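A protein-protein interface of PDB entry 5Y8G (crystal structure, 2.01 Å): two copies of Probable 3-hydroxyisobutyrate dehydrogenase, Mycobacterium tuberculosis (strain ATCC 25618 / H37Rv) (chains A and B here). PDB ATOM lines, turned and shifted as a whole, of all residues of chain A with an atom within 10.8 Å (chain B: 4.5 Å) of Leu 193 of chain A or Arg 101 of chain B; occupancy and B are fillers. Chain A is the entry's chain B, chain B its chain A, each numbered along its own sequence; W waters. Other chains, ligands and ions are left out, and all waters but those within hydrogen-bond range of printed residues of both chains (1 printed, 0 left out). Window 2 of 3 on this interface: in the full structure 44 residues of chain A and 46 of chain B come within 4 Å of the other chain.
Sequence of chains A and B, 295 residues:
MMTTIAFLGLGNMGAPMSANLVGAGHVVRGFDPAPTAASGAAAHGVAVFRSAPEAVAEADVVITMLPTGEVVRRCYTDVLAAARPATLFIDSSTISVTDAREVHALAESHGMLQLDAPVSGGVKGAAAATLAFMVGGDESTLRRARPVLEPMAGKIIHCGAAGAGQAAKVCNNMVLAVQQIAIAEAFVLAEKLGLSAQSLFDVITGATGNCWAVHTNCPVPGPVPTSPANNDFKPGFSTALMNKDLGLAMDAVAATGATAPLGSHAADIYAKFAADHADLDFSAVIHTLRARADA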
ATOM      1  N   GLU A 185     -23.154  -5.705  -0.857  1.00  0.00           N
ATOM      2  CA  GLU A 185     -23.982  -4.893  -0.002  1.00  0.00           C
ATOM      3  C   GLU A 185     -23.731  -3.389  -0.212  1.00  0.00           C
ATOM      4  O   GLU A 185     -24.677  -2.604  -0.295  1.00  0.00           O
ATOM      5  CB  GLU A 185     -23.721  -5.210   1.452  1.00  0.00           C
ATOM      6  CG  GLU A 185     -24.131  -6.611   1.916  1.00  0.00           C
ATOM      7  CD  GLU A 185     -23.762  -6.879   3.396  1.00  0.00           C
ATOM      8  OE1 GLU A 185     -23.288  -5.952   4.168  1.00  0.00           O
ATOM      9  OE2 GLU A 185     -24.007  -8.042   3.803  1.00  0.00           O
ATOM     10  N   ALA A 186     -22.470  -2.995  -0.295  1.00  0.00           N
ATOM     11  CA  ALA A 186     -22.130  -1.608  -0.541  1.00  0.00           C
ATOM     12  C   ALA A 186     -22.687  -1.108  -1.884  1.00  0.00           C
ATOM     13  O   ALA A 186     -23.197   0.012  -1.934  1.00  0.00           O
ATOM     14  CB  ALA A 186     -20.623  -1.449  -0.534  1.00  0.00           C
ATOM     15  N   PHE A 187     -22.540  -1.901  -2.976  1.00  0.00           N
ATOM     16  CA  PHE A 187     -22.995  -1.446  -4.245  1.00  0.00           C
ATOM     17  C   PHE A 187     -24.522  -1.314  -4.290  1.00  0.00           C
ATOM     18  O   PHE A 187     -25.022  -0.398  -4.937  1.00  0.00           O
ATOM     19  CB  PHE A 187     -22.500  -2.304  -5.430  1.00  0.00           C
ATOM     20  CG  PHE A 187     -21.148  -1.934  -5.928  1.00  0.00           C
ATOM     21  CD1 PHE A 187     -21.001  -0.881  -6.815  1.00  0.00           C
ATOM     22  CD2 PHE A 187     -20.016  -2.636  -5.514  1.00  0.00           C
ATOM     23  CE1 PHE A 187     -19.732  -0.521  -7.322  1.00  0.00           C
ATOM     24  CE2 PHE A 187     -18.735  -2.269  -5.977  1.00  0.00           C
ATOM     25  CZ  PHE A 187     -18.606  -1.176  -6.850  1.00  0.00           C
ATOM     26  N   VAL A 188     -25.257  -2.219  -3.643  1.00  0.00           N
ATOM     27  CA  VAL A 188     -26.710  -2.133  -3.600  1.00  0.00           C
ATOM     28  C   VAL A 188     -27.172  -0.952  -2.790  1.00  0.00           C
ATOM     29  O   VAL A 188     -28.068  -0.180  -3.244  1.00  0.00           O
ATOM     30  CB  VAL A 188     -27.360  -3.457  -3.180  1.00  0.00           C
ATOM     31  CG1 VAL A 188     -28.896  -3.321  -3.291  1.00  0.00           C
ATOM     32  CG2 VAL A 188     -26.983  -4.532  -4.203  1.00  0.00           C
ATOM     33  N   LEU A 189     -26.514  -0.723  -1.656  1.00  0.00           N
ATOM     34  CA  LEU A 189     -26.828   0.403  -0.775  1.00  0.00           C
ATOM     35  C   LEU A 189     -26.592   1.696  -1.521  1.00  0.00           C
ATOM     36  O   LEU A 189     -27.448   2.571  -1.505  1.00  0.00           O
ATOM     37  CB  LEU A 189     -26.077   0.338   0.546  1.00  0.00           C
ATOM     38  CG  LEU A 189     -26.332   1.521   1.490  1.00  0.00           C
ATOM     39  CD1 LEU A 189     -27.792   1.622   1.988  1.00  0.00           C
ATOM     40  CD2 LEU A 189     -25.360   1.413   2.659  1.00  0.00           C
ATOM     41  N   ALA A 190     -25.457   1.796  -2.216  1.00  0.00           N
ATOM     42  CA  ALA A 190     -25.149   2.947  -3.056  1.00  0.00           C
ATOM     43  C   ALA A 190     -26.256   3.197  -4.046  1.00  0.00           C
ATOM     44  O   ALA A 190     -26.650   4.331  -4.202  1.00  0.00           O
ATOM     45  CB  ALA A 190     -23.854   2.765  -3.816  1.00  0.00           C
ATOM     46  N   GLU A 191     -26.691   2.169  -4.770  1.00  0.00           N
ATOM     47  CA  GLU A 191     -27.733   2.321  -5.753  1.00  0.00           C
ATOM     48  C   GLU A 191     -28.978   2.856  -5.081  1.00  0.00           C
ATOM     49  O   GLU A 191     -29.628   3.725  -5.621  1.00  0.00           O
ATOM     50  CB  GLU A 191     -28.037   0.999  -6.486  1.00  0.00           C
ATOM     51  CG  GLU A 191     -29.227   1.049  -7.459  1.00  0.00           C
ATOM     52  N   LYS A 192     -29.309   2.375  -3.908  1.00  0.00           N
ATOM     53  CA  LYS A 192     -30.511   2.887  -3.242  1.00  0.00           C
ATOM     54  C   LYS A 192     -30.346   4.342  -2.725  1.00  0.00           C
ATOM     55  O   LYS A 192     -31.319   5.049  -2.555  1.00  0.00           O
ATOM     56  CB  LYS A 192     -30.991   1.962  -2.130  1.00  0.00           C
ATOM     57  CG  LYS A 192     -31.462   0.567  -2.660  1.00  0.00           C
ATOM     58  CD  LYS A 192     -31.804  -0.319  -1.486  1.00  0.00           C
ATOM     59  CE  LYS A 192     -32.889  -1.345  -1.775  1.00  0.00           C
ATOM     60  NZ  LYS A 192     -32.311  -2.528  -2.440  1.00  0.00           N
ATOM     61  N   LEU A 193     -29.113   4.763  -2.471  1.00  0.00           N
ATOM     62  CA  LEU A 193     -28.841   6.086  -1.988  1.00  0.00           C
ATOM     63  C   LEU A 193     -28.703   7.078  -3.124  1.00  0.00           C
ATOM     64  O   LEU A 193     -28.506   8.248  -2.849  1.00  0.00           O
ATOM     65  CB  LEU A 193     -27.578   6.098  -1.098  1.00  0.00           C
ATOM     66  CG  LEU A 193     -27.749   5.463   0.269  1.00  0.00           C
ATOM     67  CD1 LEU A 193     -26.402   5.280   0.960  1.00  0.00           C
ATOM     68  CD2 LEU A 193     -28.736   6.195   1.205  1.00  0.00           C
ATOM     69  N   GLY A 194     -28.798   6.628  -4.375  1.00  0.00           N
ATOM     70  CA  GLY A 194     -28.449   7.407  -5.557  1.00  0.00           C
ATOM     71  C   GLY A 194     -26.979   7.674  -5.843  1.00  0.00           C
ATOM     72  O   GLY A 194     -26.660   8.599  -6.605  1.00  0.00           O
ATOM     73  N   LEU A 195     -26.070   6.893  -5.256  1.00  0.00           N
ATOM     74  CA  LEU A 195     -24.659   7.031  -5.572  1.00  0.00           C
ATOM     75  C   LEU A 195     -24.369   6.100  -6.786  1.00  0.00           C
ATOM     76  O   LEU A 195     -24.740   4.957  -6.727  1.00  0.00           O
ATOM     77  CB  LEU A 195     -23.849   6.685  -4.335  1.00  0.00           C
ATOM     78  CG  LEU A 195     -22.339   6.572  -4.504  1.00  0.00           C
ATOM     79  CD1 LEU A 195     -21.749   7.918  -4.844  1.00  0.00           C
ATOM     80  CD2 LEU A 195     -21.786   6.050  -3.230  1.00  0.00           C
ATOM     81  N   SER A 196     -23.768   6.578  -7.881  1.00  0.00           N
ATOM     82  CA  SER A 196     -23.484   5.678  -9.052  1.00  0.00           C
ATOM     83  C   SER A 196     -22.448   4.569  -8.758  1.00  0.00           C
ATOM     84  O   SER A 196     -21.594   4.700  -7.832  1.00  0.00           O
ATOM     85  CB  SER A 196     -22.998   6.449 -10.293  1.00  0.00           C
ATOM     86  OG  SER A 196     -21.637   6.895 -10.153  1.00  0.00           O
ATOM     87  N   ALA A 197     -22.572   3.476  -9.519  1.00  0.00           N
ATOM     88  CA  ALA A 197     -21.700   2.321  -9.371  1.00  0.00           C
ATOM     89  C   ALA A 197     -20.307   2.760  -9.679  1.00  0.00           C
ATOM     90  O   ALA A 197     -19.370   2.393  -8.960  1.00  0.00           O
ATOM     91  CB  ALA A 197     -22.088   1.233 -10.347  1.00  0.00           C
ATOM     92  N   SER A 199     -19.012   5.738  -9.368  1.00  0.00           N
ATOM     93  CA  SER A 199     -18.466   6.620  -8.305  1.00  0.00           C
ATOM     94  C   SER A 199     -18.080   5.839  -7.082  1.00  0.00           C
ATOM     95  O   SER A 199     -17.008   6.043  -6.534  1.00  0.00           O
ATOM     96  CB  SER A 199     -19.476   7.655  -7.816  1.00  0.00           C
ATOM     97  OG  SER A 199     -19.850   8.449  -8.895  1.00  0.00           O
ATOM     98  N   LEU A 200     -18.947   4.915  -6.664  1.00  0.00           N
ATOM     99  CA  LEU A 200     -18.589   4.057  -5.543  1.00  0.00           C
ATOM    100  C   LEU A 200     -17.335   3.248  -5.853  1.00  0.00           C
ATOM    101  O   LEU A 200     -16.461   3.126  -5.037  1.00  0.00           O
ATOM    102  CB  LEU A 200     -19.784   3.169  -5.136  1.00  0.00           C
ATOM    103  CG  LEU A 200     -19.321   2.238  -3.991  1.00  0.00           C
ATOM    104  CD1 LEU A 200     -19.191   3.002  -2.702  1.00  0.00           C
ATOM    105  CD2 LEU A 200     -20.230   1.021  -3.810  1.00  0.00           C
ATOM    106  N   VAL B  97     -26.965  10.742   4.906  1.00  0.00           N
ATOM    107  CA  VAL B  97     -27.246  11.175   3.545  1.00  0.00           C
ATOM    108  C   VAL B  97     -28.485  12.045   3.550  1.00  0.00           C
ATOM    109  O   VAL B  97     -28.494  13.080   2.886  1.00  0.00           O
ATOM    110  CB  VAL B  97     -27.371   9.965   2.584  1.00  0.00           C
ATOM    111  CG1 VAL B  97     -27.817  10.367   1.191  1.00  0.00           C
ATOM    112  CG2 VAL B  97     -26.052   9.190   2.525  1.00  0.00           C
ATOM    113  N   THR B  98     -29.552  11.590   4.235  1.00  0.00           N
ATOM    114  CA  THR B  98     -30.798  12.360   4.349  1.00  0.00           C
ATOM    115  C   THR B  98     -30.562  13.767   4.883  1.00  0.00           C
ATOM    116  O   THR B  98     -31.051  14.766   4.307  1.00  0.00           O
ATOM    117  CB  THR B  98     -31.788  11.641   5.292  1.00  0.00           C
ATOM    118  OG1 THR B  98     -31.963  10.311   4.832  1.00  0.00           O
ATOM    119  CG2 THR B  98     -33.187  12.283   5.228  1.00  0.00           C
ATOM    120  N   ASP B  99     -29.832  13.841   6.001  1.00  0.00           N
ATOM    121  CA  ASP B  99     -29.480  15.159   6.613  1.00  0.00           C
ATOM    122  C   ASP B  99     -28.650  16.028   5.678  1.00  0.00           C
ATOM    123  O   ASP B  99     -28.972  17.185   5.507  1.00  0.00           O
ATOM    124  CB  ASP B  99     -28.796  15.002   7.964  1.00  0.00           C
ATOM    125  CG  ASP B  99     -29.741  14.511   9.050  1.00  0.00           C
ATOM    126  OD1 ASP B  99     -30.978  14.508   8.854  1.00  0.00           O
ATOM    127  OD2 ASP B  99     -29.238  14.142  10.141  1.00  0.00           O
ATOM    128  N   ALA B 100     -27.665  15.418   4.991  1.00  0.00           N
ATOM    129  CA  ALA B 100     -26.880  16.128   4.061  1.00  0.00           C
ATOM    130  C   ALA B 100     -27.706  16.782   3.005  1.00  0.00           C
ATOM    131  O   ALA B 100     -27.503  17.966   2.695  1.00  0.00           O
ATOM    132  CB  ALA B 100     -25.857  15.198   3.390  1.00  0.00           C
ATOM    133  N   ARG B 101     -28.586  16.027   2.386  1.00  0.00           N
ATOM    134  CA  ARG B 101     -29.449  16.528   1.338  1.00  0.00           C
ATOM    135  C   ARG B 101     -30.440  17.602   1.827  1.00  0.00           C
ATOM    136  O   ARG B 101     -30.693  18.527   1.129  1.00  0.00           O
ATOM    137  CB  ARG B 101     -30.131  15.403   0.579  1.00  0.00           C
ATOM    138  CG  ARG B 101     -29.185  14.579  -0.270  1.00  0.00           C
ATOM    139  CD  ARG B 101     -29.762  13.275  -0.787  1.00  0.00           C
ATOM    140  NE  ARG B 101     -28.851  12.657  -1.715  1.00  0.00           N
ATOM    141  CZ  ARG B 101     -28.855  11.394  -2.104  1.00  0.00           C
ATOM    142  NH1 ARG B 101     -29.739  10.553  -1.657  1.00  0.00           N
ATOM    143  NH2 ARG B 101     -27.959  10.999  -2.961  1.00  0.00           N
ATOM    144  N   GLU B 102     -30.982  17.440   3.025  1.00  0.00           N
ATOM    145  CA  GLU B 102     -31.869  18.457   3.577  1.00  0.00           C
ATOM    146  C   GLU B 102     -31.086  19.784   3.768  1.00  0.00           C
ATOM    147  O   GLU B 102     -31.577  20.833   3.362  1.00  0.00           O
ATOM    148  CB  GLU B 102     -32.464  17.989   4.874  1.00  0.00           C
ATOM    149  CG  GLU B 102     -33.300  19.045   5.594  1.00  0.00           C
ATOM    150  CD  GLU B 102     -33.622  18.692   7.066  1.00  0.00           C
ATOM    151  OE1 GLU B 102     -34.272  19.529   7.764  1.00  0.00           O
ATOM    152  OE2 GLU B 102     -33.195  17.615   7.557  1.00  0.00           O
ATOM    153  N   VAL B 103     -29.904  19.766   4.385  1.00  0.00           N
ATOM    154  CA  VAL B 103     -29.169  21.023   4.558  1.00  0.00           C
ATOM    155  C   VAL B 103     -28.660  21.661   3.245  1.00  0.00           C
ATOM    156  O   VAL B 103     -28.575  22.895   3.104  1.00  0.00           O
ATOM    157  CB  VAL B 103     -28.049  20.936   5.609  1.00  0.00           C
ATOM    158  CG1 VAL B 103     -28.575  20.476   6.984  1.00  0.00           C
ATOM    159  CG2 VAL B 103     -26.896  20.064   5.153  1.00  0.00           C
ATOM    160  N   HIS B 104     -28.371  20.812   2.247  1.00  0.00           N
ATOM    161  CA  HIS B 104     -28.001  21.266   0.945  1.00  0.00           C
ATOM    162  C   HIS B 104     -29.167  22.072   0.349  1.00  0.00           C
ATOM    163  O   HIS B 104     -28.984  23.200  -0.068  1.00  0.00           O
ATOM    164  CB  HIS B 104     -27.599  20.087   0.039  1.00  0.00           C
ATOM    165  CG  HIS B 104     -27.372  20.482  -1.370  1.00  0.00           C
ATOM    166  ND1 HIS B 104     -26.186  21.039  -1.799  1.00  0.00           N
ATOM    167  CD2 HIS B 104     -28.203  20.462  -2.445  1.00  0.00           C
ATOM    168  CE1 HIS B 104     -26.299  21.346  -3.078  1.00  0.00           C
ATOM    169  NE2 HIS B 104     -27.517  21.033  -3.477  1.00  0.00           N
ATOM    170  N   ALA B 105     -30.352  21.484   0.326  1.00  0.00           N
ATOM    171  CA  ALA B 105     -31.524  22.136  -0.189  1.00  0.00           C
ATOM    172  C   ALA B 105     -31.822  23.436   0.590  1.00  0.00           C
ATOM    173  O   ALA B 105     -32.176  24.468   0.007  1.00  0.00           O
ATOM    174  CB  ALA B 105     -32.740  21.207  -0.134  1.00  0.00           C
ATOM    175  N   ALA B 162     -25.436  16.193  -4.504  1.00  0.00           N
ATOM    176  CA  ALA B 162     -25.525  16.420  -3.065  1.00  0.00           C
ATOM    177  C   ALA B 162     -25.944  15.154  -2.338  1.00  0.00           C
ATOM    178  O   ALA B 162     -26.872  14.459  -2.736  1.00  0.00           O
ATOM    179  CB  ALA B 162     -26.539  17.525  -2.781  1.00  0.00           C
ATOM    180  N   GLY B 163     -25.227  14.859  -1.272  1.00  0.00           N
ATOM    181  CA  GLY B 163     -25.309  13.631  -0.515  1.00  0.00           C
ATOM    182  C   GLY B 163     -24.387  12.465  -0.926  1.00  0.00           C
ATOM    183  O   GLY B 163     -24.160  11.532  -0.139  1.00  0.00           O
ATOM    184  N   ALA B 164     -23.872  12.495  -2.150  1.00  0.00           N
ATOM    185  CA  ALA B 164     -22.987  11.455  -2.626  1.00  0.00           C
ATOM    186  C   ALA B 164     -21.702  11.320  -1.818  1.00  0.00           C
ATOM    187  O   ALA B 164     -21.124  10.226  -1.736  1.00  0.00           O
ATOM    188  CB  ALA B 164     -22.628  11.690  -4.102  1.00  0.00           C
ATOM    189  N   ALA B 167     -22.587   9.420   1.188  1.00  0.00           N
ATOM    190  CA  ALA B 167     -22.910   8.033   0.850  1.00  0.00           C
ATOM    191  C   ALA B 167     -21.614   7.264   0.553  1.00  0.00           C
ATOM    192  O   ALA B 167     -21.488   6.095   0.942  1.00  0.00           O
ATOM    193  CB  ALA B 167     -23.803   7.985  -0.408  1.00  0.00           C
ATOM    194  N   ALA B 252     -28.769   4.693   6.991  1.00  0.00           N
ATOM    195  CA  ALA B 252     -28.909   4.642   5.597  1.00  0.00           C
ATOM    196  C   ALA B 252     -29.608   3.332   5.144  1.00  0.00           C
ATOM    197  O   ALA B 252     -30.467   3.360   4.240  1.00  0.00           O
ATOM    198  CB  ALA B 252     -27.562   4.771   4.935  1.00  0.00           C
ATOM    199  N   THR B 256     -33.387   3.267   3.360  1.00  0.00           N
ATOM    200  CA  THR B 256     -33.599   2.731   2.010  1.00  0.00           C
ATOM    201  C   THR B 256     -34.298   1.385   1.944  1.00  0.00           C
ATOM    202  O   THR B 256     -34.639   0.937   0.875  1.00  0.00           O
ATOM    203  CB  THR B 256     -32.246   2.570   1.281  1.00  0.00           C
ATOM    204  OG1 THR B 256     -31.408   1.748   2.079  1.00  0.00           O
ATOM    205  CG2 THR B 256     -31.597   3.968   1.111  1.00  0.00           C
HETATM  206  O   HOH W   1     -31.584   7.791  -2.263  1.00  0.00           O
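NE of Arg 101 of chain B lies within hydrogen-bond range of O of Ala 162 of chain B (2.9 Å). The backbone carbonyl oxygen (O) of Ala 252 of chain B is in hydrogen-bond range of the side-chain hydroxyl (OG1) of Thr 256 of chain B (2.9 Å). N of Leu 195 of chain A is in hydrogen-bond range of O of Ala 190 of chain A.
Hydrophobic or aromatic side chains of chain A within 4 Å of the printed part of chain B: Leu 189, Leu 193 and Leu 195. Hydrophobic or aromatic side chains of chain B within 4 Å of the printed part of chain A: Ala 164 and Ala 167. Among the printed residues, no Asp or Glu carboxylate lies within 4 Å of a Lys or Arg side-chain nitrogen of the other chain.
The backbone carbonyl oxygen (O) of Leu 193 of chain A sits at hydrogen-bond distance from the guanidinium group (NH2) of Arg 101 of chain B.
No position is printed for both chains.
Of the printed residues of chain B, Lys 192 of chain A touches Thr 256 (3.7 Å). Of the printed residues of chain B, Leu 193 of chain A touches Arg 101 (2.8 Å), Ala 167 (3.99 Å) and Thr 256 (3.6 Å). Of the printed residues of chain B, Leu 195 of chain A touches Ala 164 and Ala 167. No residue of chain A comes within 4 Å of Val 97 of chain B. No residue of chain A comes within 4 Å of Thr 98 of chain B. Of the printed residues of chain A, Arg 101 of chain B touches Leu 193 (2.8 Å). No residue of chain A comes within 4 Å of His 104 of chain B. No residue of chain A comes within 4 Å of Ala 105 of chain B. Ala 162 of chain B touches none of the printed residues of chain A. No residue of chain A comes within 4 Å of Gly 163 of chain B. Printed residues of chain A within 4 Å of Ala 167 of chain B: Leu 193 and Leu 195. Of chain A, only Leu 189 comes within 4 Å of Ala 252 of chain B. Of the printed residues of chain A, Thr 256 of chain B touches Leu 189, Lys 192 and Leu 193. The nearest residue of chain A that does not touch Arg 101 of chain B is Gly 194 of chain A (4.5 Å).
Among the printed residues, merely in contact across the chains: Leu 189 of chain A with Thr 256 of chain B (3.6 Å), Leu 193 of chain A with Thr 256 of chain B (3.6 Å), Lys 192 of chain A with Thr 256 of chain B (3.7 Å), Leu 189 of chain A with Ala 252 of chain B (3.9 Å), Leu 195 of chain A with Ala 164 of chain B (3.9 Å), Leu 195 of chain A with Ala 167 of chain B (3.97 Å) and Leu 193 of chain A with Ala 167 of chain B (3.99 Å).
Water W1 lies within hydrogen-bond range of O of Lys 192 of chain A (2.8 Å), O of Leu 193 of chain A (3.2 Å) and NH1 of Arg 101 of chain B (3.4 Å).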
